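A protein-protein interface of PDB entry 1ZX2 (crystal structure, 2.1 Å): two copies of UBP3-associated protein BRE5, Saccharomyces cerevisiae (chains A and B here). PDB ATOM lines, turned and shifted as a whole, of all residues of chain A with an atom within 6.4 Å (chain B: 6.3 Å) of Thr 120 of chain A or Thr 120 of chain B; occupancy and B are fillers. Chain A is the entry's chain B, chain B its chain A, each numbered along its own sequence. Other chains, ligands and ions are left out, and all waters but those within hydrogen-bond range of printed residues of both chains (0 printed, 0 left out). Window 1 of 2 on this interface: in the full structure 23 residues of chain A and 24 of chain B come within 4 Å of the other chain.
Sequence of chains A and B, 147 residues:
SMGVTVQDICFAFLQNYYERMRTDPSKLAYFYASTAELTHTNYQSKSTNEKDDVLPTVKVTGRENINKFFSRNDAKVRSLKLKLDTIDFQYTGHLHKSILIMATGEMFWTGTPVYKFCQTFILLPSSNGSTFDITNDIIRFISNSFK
The backbone NH (N) of Thr 120 of chain B sits at hydrogen-bond distance from the backbone carbonyl oxygen (O) of Ile 138 of chain B (2.9 Å). N of Ile 122 of chain A is in hydrogen-bond range of O of Asn 136 of chain A (3.0 Å). O of Ile 138 of chain A is in hydrogen-bond range of N of Thr 120 of chain A, 2.8 Å away. The side-chain amide oxygen (OE1) of Gln 119 of chain A sits close to the side-chain carboxylate (OD1) of Asp 137 of chain A (2.9 Å). The backbone NH (N) of Gln 119 of chain A is in hydrogen-bond range of the backbone carbonyl oxygen (O) of Ala 103 of chain A, at 2.7 Å. The backbone NH of Ile 122 of chain B is in hydrogen-bond range of the backbone carbonyl oxygen of Asn 136 of chain B.
Thr 120 of chain A touches just these residues of chain B: Met 102 and Thr 120. Of the printed residues of chain A, Thr 120 of chain B touches Met 102 (3.2 Å) and Thr 120 (3.0 Å). Of the printed residues of chain A, Cys 118 of chain B touches Met 102 and Cys 118. Of the printed residues of chain B, Ile 122 of chain A touches Leu 100 and Ile 122. Asp 137 of chain B touches none of the printed residues of chain A. Phe 121 of chain A touches none of the printed residues of chain B. The nearest residue of chain B that does not touch Thr 120 of chain A is Leu 100 of chain B (4.1 Å).
Among the printed residues, merely in contact across the chains: Leu 100 of chain A with Ile 122 of chain B, Leu 100 of chain A with Asn 136 of chain B, Leu 100 of chain A with Ile 138 of chain B, Met 102 of chain A with Cys 118 of chain B, Met 102 of chain A with Ile 138 of chain B, Cys 118 of chain A with Met 102 of chain B, Gln 119 of chain A with Met 102 of chain B, Thr 120 of chain A with Thr 120 of chain B, Ile 122 of chain A with Leu 100 of chain B, Ile 122 of chain A with Ile 122 of chain B, Asn 136 of chain A with Leu 100 of chain B, Ile 138 of chain A with Leu 100 of chain B and Ile 138 of chain A with Met 102 of chain B.
The side-chain sulfur (SD) of Met 102 of chain B sits close to the side-chain hydroxyl (OG1) of Thr 120 of chain A (3.8 Å). OG1 of Thr 120 of chain B lies within hydrogen-bond range of SD of Met 102 of chain A, at 3.2 Å. SG of Cys 118 of chain A sits close to SG of Cys 118 of chain B (3.7 Å).
Of the 13 printed residues of chain B, 7 touch a printed residue of chain A. Printed residues of chain B that touch a printed residue of chain A: Leu 100, Met 102, Cys 118, Thr 120, Ile 122, Asn 136 and Ile 138. Hydrophobic or aromatic side chains of chain B within 4 Å of the printed part of chain A: Leu 100, Met 102, Ile 122 and Ile 138. Of the 13 printed residues of chain A, 8 touch a printed residue of chain B. Printed residues of chain A that touch a printed residue of chain B: Leu 100, Met 102, Cys 118, Gln 119, Thr 120, Ile 122, Asn 136 and Ile 138. Among the printed residues, 16 pairs touch across the chains. Among the printed residues, no Asp or Glu carboxylate lies within 4 Å of a Lys or Arg side-chain nitrogen of the other chain.
Leu 100 of chain A touches Ile 138 of chain B, and with the chains exchanged Ile 138 of chain A touches Leu 100 of chain B. Met 102 of chain A touches Cys 118 of chain B, and with the chains exchanged Cys 118 of chain A touches Met 102 of chain B. Met 102 of chain A touches Ile 138 of chain B, and with the chains exchanged Ile 138 of chain A touches Met 102 of chain B. Cys 118 of chain B touches its own counterpart, Cys 118 of chain A. Positions printed for both chains: 100, 101, 102, 103, 118, 119, 120, 121, 122, 136, 137, 138 and 139.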
ATOM      1  N   LEU A 100      24.339  -9.802  -7.748  1.00  0.00           N
ATOM      2  CA  LEU A 100      23.117  -9.062  -7.591  1.00  0.00           C
ATOM      3  C   LEU A 100      23.170  -8.306  -6.303  1.00  0.00           C
ATOM      4  O   LEU A 100      23.462  -8.830  -5.259  1.00  0.00           O
ATOM      5  CB  LEU A 100      22.012 -10.062  -7.429  1.00  0.00           C
ATOM      6  CG  LEU A 100      20.553  -9.738  -7.468  1.00  0.00           C
ATOM      7  CD1 LEU A 100      19.557 -10.693  -6.709  1.00  0.00           C
ATOM      8  CD2 LEU A 100      19.999  -8.460  -8.024  1.00  0.00           C
ATOM      9  N   ILE A 101      22.848  -7.032  -6.380  1.00  0.00           N
ATOM     10  CA  ILE A 101      22.755  -6.123  -5.219  1.00  0.00           C
ATOM     11  C   ILE A 101      21.325  -5.560  -5.187  1.00  0.00           C
ATOM     12  O   ILE A 101      20.832  -5.060  -6.214  1.00  0.00           O
ATOM     13  CB  ILE A 101      23.730  -4.964  -5.407  1.00  0.00           C
ATOM     14  CG1 ILE A 101      25.152  -5.512  -5.556  1.00  0.00           C
ATOM     15  CG2 ILE A 101      23.760  -4.103  -4.174  1.00  0.00           C
ATOM     16  CD1 ILE A 101      26.244  -4.473  -5.862  1.00  0.00           C
ATOM     17  N   MET A 102      20.730  -5.516  -4.015  1.00  0.00           N
ATOM     18  CA  MET A 102      19.520  -4.739  -3.805  1.00  0.00           C
ATOM     19  C   MET A 102      19.785  -3.812  -2.652  1.00  0.00           C
ATOM     20  O   MET A 102      20.218  -4.297  -1.573  1.00  0.00           O
ATOM     21  CB  MET A 102      18.354  -5.675  -3.448  1.00  0.00           C
ATOM     22  CG  MET A 102      16.953  -5.012  -3.487  1.00  0.00           C
ATOM     23  SD  MET A 102      15.469  -6.157  -3.122  1.00  0.00           S
ATOM     24  CE  MET A 102      15.418  -5.695  -1.459  1.00  0.00           C
ATOM     25  N   ALA A 103      19.520  -2.514  -2.899  1.00  0.00           N
ATOM     26  CA  ALA A 103      19.591  -1.456  -1.918  1.00  0.00           C
ATOM     27  C   ALA A 103      18.271  -0.699  -1.823  1.00  0.00           C
ATOM     28  O   ALA A 103      17.565  -0.491  -2.829  1.00  0.00           O
ATOM     29  CB  ALA A 103      20.718  -0.483  -2.240  1.00  0.00           C
ATOM     30  N   CYS A 118      14.458   2.228  -4.159  1.00  0.00           N
ATOM     31  CA  CYS A 118      14.739   0.805  -4.243  1.00  0.00           C
ATOM     32  C   CYS A 118      15.586   0.676  -5.496  1.00  0.00           C
ATOM     33  O   CYS A 118      15.199   1.207  -6.573  1.00  0.00           O
ATOM     34  CB  CYS A 118      13.480  -0.035  -4.381  1.00  0.00           C
ATOM     35  SG  CYS A 118      12.378   0.120  -2.929  1.00  0.00           S
ATOM     36  N   GLN A 119      16.732   0.014  -5.369  1.00  0.00           N
ATOM     37  CA  GLN A 119      17.632  -0.084  -6.504  1.00  0.00           C
ATOM     38  C   GLN A 119      18.161  -1.455  -6.595  1.00  0.00           C
ATOM     39  O   GLN A 119      18.541  -2.028  -5.553  1.00  0.00           O
ATOM     40  CB  GLN A 119      18.784   0.938  -6.333  1.00  0.00           C
ATOM     41  CG  GLN A 119      19.847   0.963  -7.486  1.00  0.00           C
ATOM     42  CD  GLN A 119      20.598   2.278  -7.664  1.00  0.00           C
ATOM     43  OE1 GLN A 119      20.861   2.714  -8.822  1.00  0.00           O
ATOM     44  NE2 GLN A 119      21.046   2.843  -6.577  1.00  0.00           N
ATOM     45  N   THR A 120      18.292  -1.996  -7.788  1.00  0.00           N
ATOM     46  CA  THR A 120      19.019  -3.242  -7.904  1.00  0.00           C
ATOM     47  C   THR A 120      20.074  -3.030  -8.948  1.00  0.00           C
ATOM     48  O   THR A 120      19.787  -2.391  -9.971  1.00  0.00           O
ATOM     49  CB  THR A 120      18.149  -4.449  -8.350  1.00  0.00           C
ATOM     50  OG1 THR A 120      17.268  -4.021  -9.398  1.00  0.00           O
ATOM     51  CG2 THR A 120      17.135  -4.813  -7.357  1.00  0.00           C
ATOM     52  N   PHE A 121      21.219  -3.685  -8.772  1.00  0.00           N
ATOM     53  CA  PHE A 121      22.248  -3.787  -9.770  1.00  0.00           C
ATOM     54  C   PHE A 121      22.574  -5.220 -10.029  1.00  0.00           C
ATOM     55  O   PHE A 121      22.600  -6.019  -9.121  1.00  0.00           O
ATOM     56  CB  PHE A 121      23.568  -3.212  -9.195  1.00  0.00           C
ATOM     57  CG  PHE A 121      23.561  -1.715  -8.865  1.00  0.00           C
ATOM     58  CD1 PHE A 121      23.408  -1.297  -7.559  1.00  0.00           C
ATOM     59  CD2 PHE A 121      23.731  -0.745  -9.852  1.00  0.00           C
ATOM     60  CE1 PHE A 121      23.453   0.049  -7.228  1.00  0.00           C
ATOM     61  CE2 PHE A 121      23.784   0.643  -9.501  1.00  0.00           C
ATOM     62  CZ  PHE A 121      23.672   1.013  -8.216  1.00  0.00           C
ATOM     63  N   ILE A 122      23.021  -5.499 -11.246  1.00  0.00           N
ATOM     64  CA  ILE A 122      23.834  -6.672 -11.572  1.00  0.00           C
ATOM     65  C   ILE A 122      25.193  -6.270 -12.052  1.00  0.00           C
ATOM     66  O   ILE A 122      25.303  -5.440 -12.981  1.00  0.00           O
ATOM     67  CB  ILE A 122      23.080  -7.573 -12.618  1.00  0.00           C
ATOM     68  CG1 ILE A 122      21.851  -8.168 -11.900  1.00  0.00           C
ATOM     69  CG2 ILE A 122      23.926  -8.727 -12.963  1.00  0.00           C
ATOM     70  CD1 ILE A 122      20.862  -8.945 -12.721  1.00  0.00           C
ATOM     71  N   ASN A 136      23.034  -4.099 -15.423  1.00  0.00           N
ATOM     72  CA  ASN A 136      21.653  -3.873 -15.152  1.00  0.00           C
ATOM     73  C   ASN A 136      21.569  -2.952 -13.966  1.00  0.00           C
ATOM     74  O   ASN A 136      22.136  -3.194 -12.933  1.00  0.00           O
ATOM     75  CB  ASN A 136      20.884  -5.226 -14.819  1.00  0.00           C
ATOM     76  CG  ASN A 136      20.773  -6.116 -15.961  1.00  0.00           C
ATOM     77  OD1 ASN A 136      19.767  -6.056 -16.779  1.00  0.00           O
ATOM     78  ND2 ASN A 136      21.800  -6.936 -16.156  1.00  0.00           N
ATOM     79  N   ASP A 137      20.723  -1.948 -14.076  1.00  0.00           N
ATOM     80  CA  ASP A 137      20.476  -1.026 -12.982  1.00  0.00           C
ATOM     81  C   ASP A 137      18.981  -0.692 -13.076  1.00  0.00           C
ATOM     82  O   ASP A 137      18.553  -0.186 -14.081  1.00  0.00           O
ATOM     83  CB  ASP A 137      21.376   0.191 -13.218  1.00  0.00           C
ATOM     84  CG  ASP A 137      21.207   1.340 -12.203  1.00  0.00           C
ATOM     85  OD1 ASP A 137      20.363   1.277 -11.306  1.00  0.00           O
ATOM     86  OD2 ASP A 137      21.929   2.385 -12.262  1.00  0.00           O
ATOM     87  N   ILE A 138      18.205  -0.914 -12.016  1.00  0.00           N
ATOM     88  CA  ILE A 138      16.836  -0.463 -11.931  1.00  0.00           C
ATOM     89  C   ILE A 138      16.749   0.314 -10.657  1.00  0.00           C
ATOM     90  O   ILE A 138      17.111  -0.211  -9.574  1.00  0.00           O
ATOM     91  CB  ILE A 138      15.859  -1.673 -11.788  1.00  0.00           C
ATOM     92  CG1 ILE A 138      15.917  -2.565 -13.020  1.00  0.00           C
ATOM     93  CG2 ILE A 138      14.432  -1.088 -11.595  1.00  0.00           C
ATOM     94  CD1 ILE A 138      15.192  -3.884 -12.915  1.00  0.00           C
ATOM     95  N   ILE A 139      16.299   1.555 -10.745  1.00  0.00           N
ATOM     96  CA  ILE A 139      16.057   2.322  -9.563  1.00  0.00           C
ATOM     97  C   ILE A 139      14.713   3.006  -9.684  1.00  0.00           C
ATOM     98  O   ILE A 139      14.464   3.696 -10.665  1.00  0.00           O
ATOM     99  CB  ILE A 139      17.189   3.348  -9.246  1.00  0.00           C
ATOM    100  CG1 ILE A 139      16.767   4.175  -8.032  1.00  0.00           C
ATOM    101  CG2 ILE A 139      17.536   4.195 -10.443  1.00  0.00           C
ATOM    102  CD1 ILE A 139      17.931   4.908  -7.197  1.00  0.00           C
ATOM    103  N   LEU B 100      15.781 -10.131 -14.826  1.00  0.00           N
ATOM    104  CA  LEU B 100      15.792  -9.465 -13.551  1.00  0.00           C
ATOM    105  C   LEU B 100      14.442  -8.755 -13.368  1.00  0.00           C
ATOM    106  O   LEU B 100      14.011  -8.036 -14.247  1.00  0.00           O
ATOM    107  CB  LEU B 100      16.904  -8.408 -13.574  1.00  0.00           C
ATOM    108  CG  LEU B 100      16.932  -7.434 -12.422  1.00  0.00           C
ATOM    109  CD1 LEU B 100      17.297  -8.163 -11.128  1.00  0.00           C
ATOM    110  CD2 LEU B 100      17.990  -6.324 -12.707  1.00  0.00           C
ATOM    111  N   ILE B 101      13.790  -8.997 -12.251  1.00  0.00           N
ATOM    112  CA  ILE B 101      12.566  -8.337 -11.832  1.00  0.00           C
ATOM    113  C   ILE B 101      12.770  -7.652 -10.530  1.00  0.00           C
ATOM    114  O   ILE B 101      13.353  -8.260  -9.605  1.00  0.00           O
ATOM    115  CB  ILE B 101      11.422  -9.408 -11.627  1.00  0.00           C
ATOM    116  CG1 ILE B 101      11.185 -10.185 -12.898  1.00  0.00           C
ATOM    117  CG2 ILE B 101      10.115  -8.773 -11.293  1.00  0.00           C
ATOM    118  CD1 ILE B 101      10.208 -11.340 -12.827  1.00  0.00           C
ATOM    119  N   MET B 102      12.245  -6.424 -10.385  1.00  0.00           N
ATOM    120  CA  MET B 102      12.189  -5.769  -9.091  1.00  0.00           C
ATOM    121  C   MET B 102      10.773  -5.328  -8.925  1.00  0.00           C
ATOM    122  O   MET B 102      10.243  -4.674  -9.824  1.00  0.00           O
ATOM    123  CB  MET B 102      13.118  -4.530  -9.018  1.00  0.00           C
ATOM    124  CG  MET B 102      13.255  -3.887  -7.603  1.00  0.00           C
ATOM    125  SD  MET B 102      14.397  -2.396  -7.536  1.00  0.00           S
ATOM    126  CE  MET B 102      13.210  -1.311  -8.096  1.00  0.00           C
ATOM    127  N   ALA B 103      10.138  -5.672  -7.820  1.00  0.00           N
ATOM    128  CA  ALA B 103       8.773  -5.267  -7.578  1.00  0.00           C
ATOM    129  C   ALA B 103       8.690  -4.636  -6.197  1.00  0.00           C
ATOM    130  O   ALA B 103       9.408  -5.066  -5.268  1.00  0.00           O
ATOM    131  CB  ALA B 103       7.817  -6.461  -7.680  1.00  0.00           C
ATOM    132  N   CYS B 118      10.188  -4.612  -0.885  1.00  0.00           N
ATOM    133  CA  CYS B 118      10.875  -4.545  -2.160  1.00  0.00           C
ATOM    134  C   CYS B 118      11.396  -5.947  -2.358  1.00  0.00           C
ATOM    135  O   CYS B 118      12.019  -6.504  -1.456  1.00  0.00           O
ATOM    136  CB  CYS B 118      12.055  -3.506  -2.134  1.00  0.00           C
ATOM    137  SG  CYS B 118      12.844  -3.427  -3.790  1.00  0.00           S
ATOM    138  N   GLN B 119      11.100  -6.533  -3.516  1.00  0.00           N
ATOM    139  CA  GLN B 119      11.541  -7.896  -3.851  1.00  0.00           C
ATOM    140  C   GLN B 119      12.167  -7.910  -5.221  1.00  0.00           C
ATOM    141  O   GLN B 119      11.615  -7.348  -6.141  1.00  0.00           O
ATOM    142  CB  GLN B 119      10.353  -8.835  -3.878  1.00  0.00           C
ATOM    143  CG  GLN B 119      10.698 -10.371  -4.122  1.00  0.00           C
ATOM    144  CD  GLN B 119       9.689 -11.291  -3.467  1.00  0.00           C
ATOM    145  OE1 GLN B 119      10.043 -12.370  -2.930  1.00  0.00           O
ATOM    146  NE2 GLN B 119       8.452 -10.938  -3.582  1.00  0.00           N
ATOM    147  N   THR B 120      13.241  -8.662  -5.358  1.00  0.00           N
ATOM    148  CA  THR B 120      13.924  -8.857  -6.593  1.00  0.00           C
ATOM    149  C   THR B 120      14.038 -10.319  -6.861  1.00  0.00           C
ATOM    150  O   THR B 120      14.335 -11.072  -5.947  1.00  0.00           O
ATOM    151  CB  THR B 120      15.347  -8.259  -6.482  1.00  0.00           C
ATOM    152  OG1 THR B 120      15.220  -6.825  -6.275  1.00  0.00           O
ATOM    153  CG2 THR B 120      15.989  -8.354  -7.810  1.00  0.00           C
ATOM    154  N   PHE B 121      13.857 -10.707  -8.115  1.00  0.00           N
ATOM    155  CA  PHE B 121      14.057 -12.067  -8.578  1.00  0.00           C
ATOM    156  C   PHE B 121      14.994 -12.043  -9.723  1.00  0.00           C
ATOM    157  O   PHE B 121      14.932 -11.135 -10.531  1.00  0.00           O
ATOM    158  CB  PHE B 121      12.738 -12.604  -9.149  1.00  0.00           C
ATOM    159  CG  PHE B 121      11.636 -12.761  -8.143  1.00  0.00           C
ATOM    160  CD1 PHE B 121      10.633 -11.809  -8.041  1.00  0.00           C
ATOM    161  CD2 PHE B 121      11.591 -13.854  -7.330  1.00  0.00           C
ATOM    162  CE1 PHE B 121       9.598 -11.935  -7.157  1.00  0.00           C
ATOM    163  CE2 PHE B 121      10.497 -14.022  -6.406  1.00  0.00           C
ATOM    164  CZ  PHE B 121       9.527 -13.078  -6.335  1.00  0.00           C
ATOM    165  N   ILE B 122      15.799 -13.100  -9.874  1.00  0.00           N
ATOM    166  CA  ILE B 122      16.394 -13.396 -11.174  1.00  0.00           C
ATOM    167  C   ILE B 122      15.836 -14.738 -11.618  1.00  0.00           C
ATOM    168  O   ILE B 122      15.862 -15.703 -10.881  1.00  0.00           O
ATOM    169  CB  ILE B 122      17.912 -13.381 -11.103  1.00  0.00           C
ATOM    170  CG1 ILE B 122      18.431 -11.976 -10.873  1.00  0.00           C
ATOM    171  CG2 ILE B 122      18.560 -13.935 -12.375  1.00  0.00           C
ATOM    172  CD1 ILE B 122      19.923 -11.823 -10.589  1.00  0.00           C
ATOM    173  N   ASN B 136      17.609 -16.446  -7.803  1.00  0.00           N
ATOM    174  CA  ASN B 136      17.841 -15.454  -6.790  1.00  0.00           C
ATOM    175  C   ASN B 136      16.572 -14.835  -6.408  1.00  0.00           C
ATOM    176  O   ASN B 136      15.772 -14.474  -7.221  1.00  0.00           O
ATOM    177  CB  ASN B 136      18.758 -14.316  -7.372  1.00  0.00           C
ATOM    178  CG  ASN B 136      20.111 -14.793  -7.706  1.00  0.00           C
ATOM    179  OD1 ASN B 136      21.069 -14.809  -6.846  1.00  0.00           O
ATOM    180  ND2 ASN B 136      20.261 -15.255  -8.941  1.00  0.00           N
ATOM    181  N   ASP B 137      16.398 -14.603  -5.117  1.00  0.00           N
ATOM    182  CA  ASP B 137      15.215 -13.985  -4.587  1.00  0.00           C
ATOM    183  C   ASP B 137      15.674 -13.241  -3.366  1.00  0.00           C
ATOM    184  O   ASP B 137      16.199 -13.861  -2.433  1.00  0.00           O
ATOM    185  CB  ASP B 137      14.289 -15.135  -4.194  1.00  0.00           C
ATOM    186  CG  ASP B 137      13.011 -14.719  -3.474  1.00  0.00           C
ATOM    187  OD1 ASP B 137      12.830 -13.563  -3.033  1.00  0.00           O
ATOM    188  OD2 ASP B 137      12.101 -15.581  -3.254  1.00  0.00           O
ATOM    189  N   ILE B 138      15.348 -11.948  -3.274  1.00  0.00           N
ATOM    190  CA  ILE B 138      15.685 -11.076  -2.103  1.00  0.00           C
ATOM    191  C   ILE B 138      14.435 -10.296  -1.835  1.00  0.00           C
ATOM    192  O   ILE B 138      13.914  -9.695  -2.767  1.00  0.00           O
ATOM    193  CB  ILE B 138      16.817 -10.046  -2.389  1.00  0.00           C
ATOM    194  CG1 ILE B 138      18.118 -10.784  -2.791  1.00  0.00           C
ATOM    195  CG2 ILE B 138      17.101  -9.220  -1.088  1.00  0.00           C
ATOM    196  CD1 ILE B 138      19.313  -9.958  -3.363  1.00  0.00           C
ATOM    197  N   ILE B 139      13.967 -10.283  -0.581  1.00  0.00           N
ATOM    198  CA  ILE B 139      12.910  -9.382  -0.182  1.00  0.00           C
ATOM    199  C   ILE B 139      13.272  -8.701   1.143  1.00  0.00           C
ATOM    200  O   ILE B 139      13.834  -9.326   2.045  1.00  0.00           O
ATOM    201  CB  ILE B 139      11.569 -10.158  -0.061  1.00  0.00           C
ATOM    202  CG1 ILE B 139      10.415  -9.194   0.181  1.00  0.00           C
ATOM    203  CG2 ILE B 139      11.646 -11.204   1.072  1.00  0.00           C
ATOM    204  CD1 ILE B 139       9.015  -9.840   0.106  1.00  0.00           C
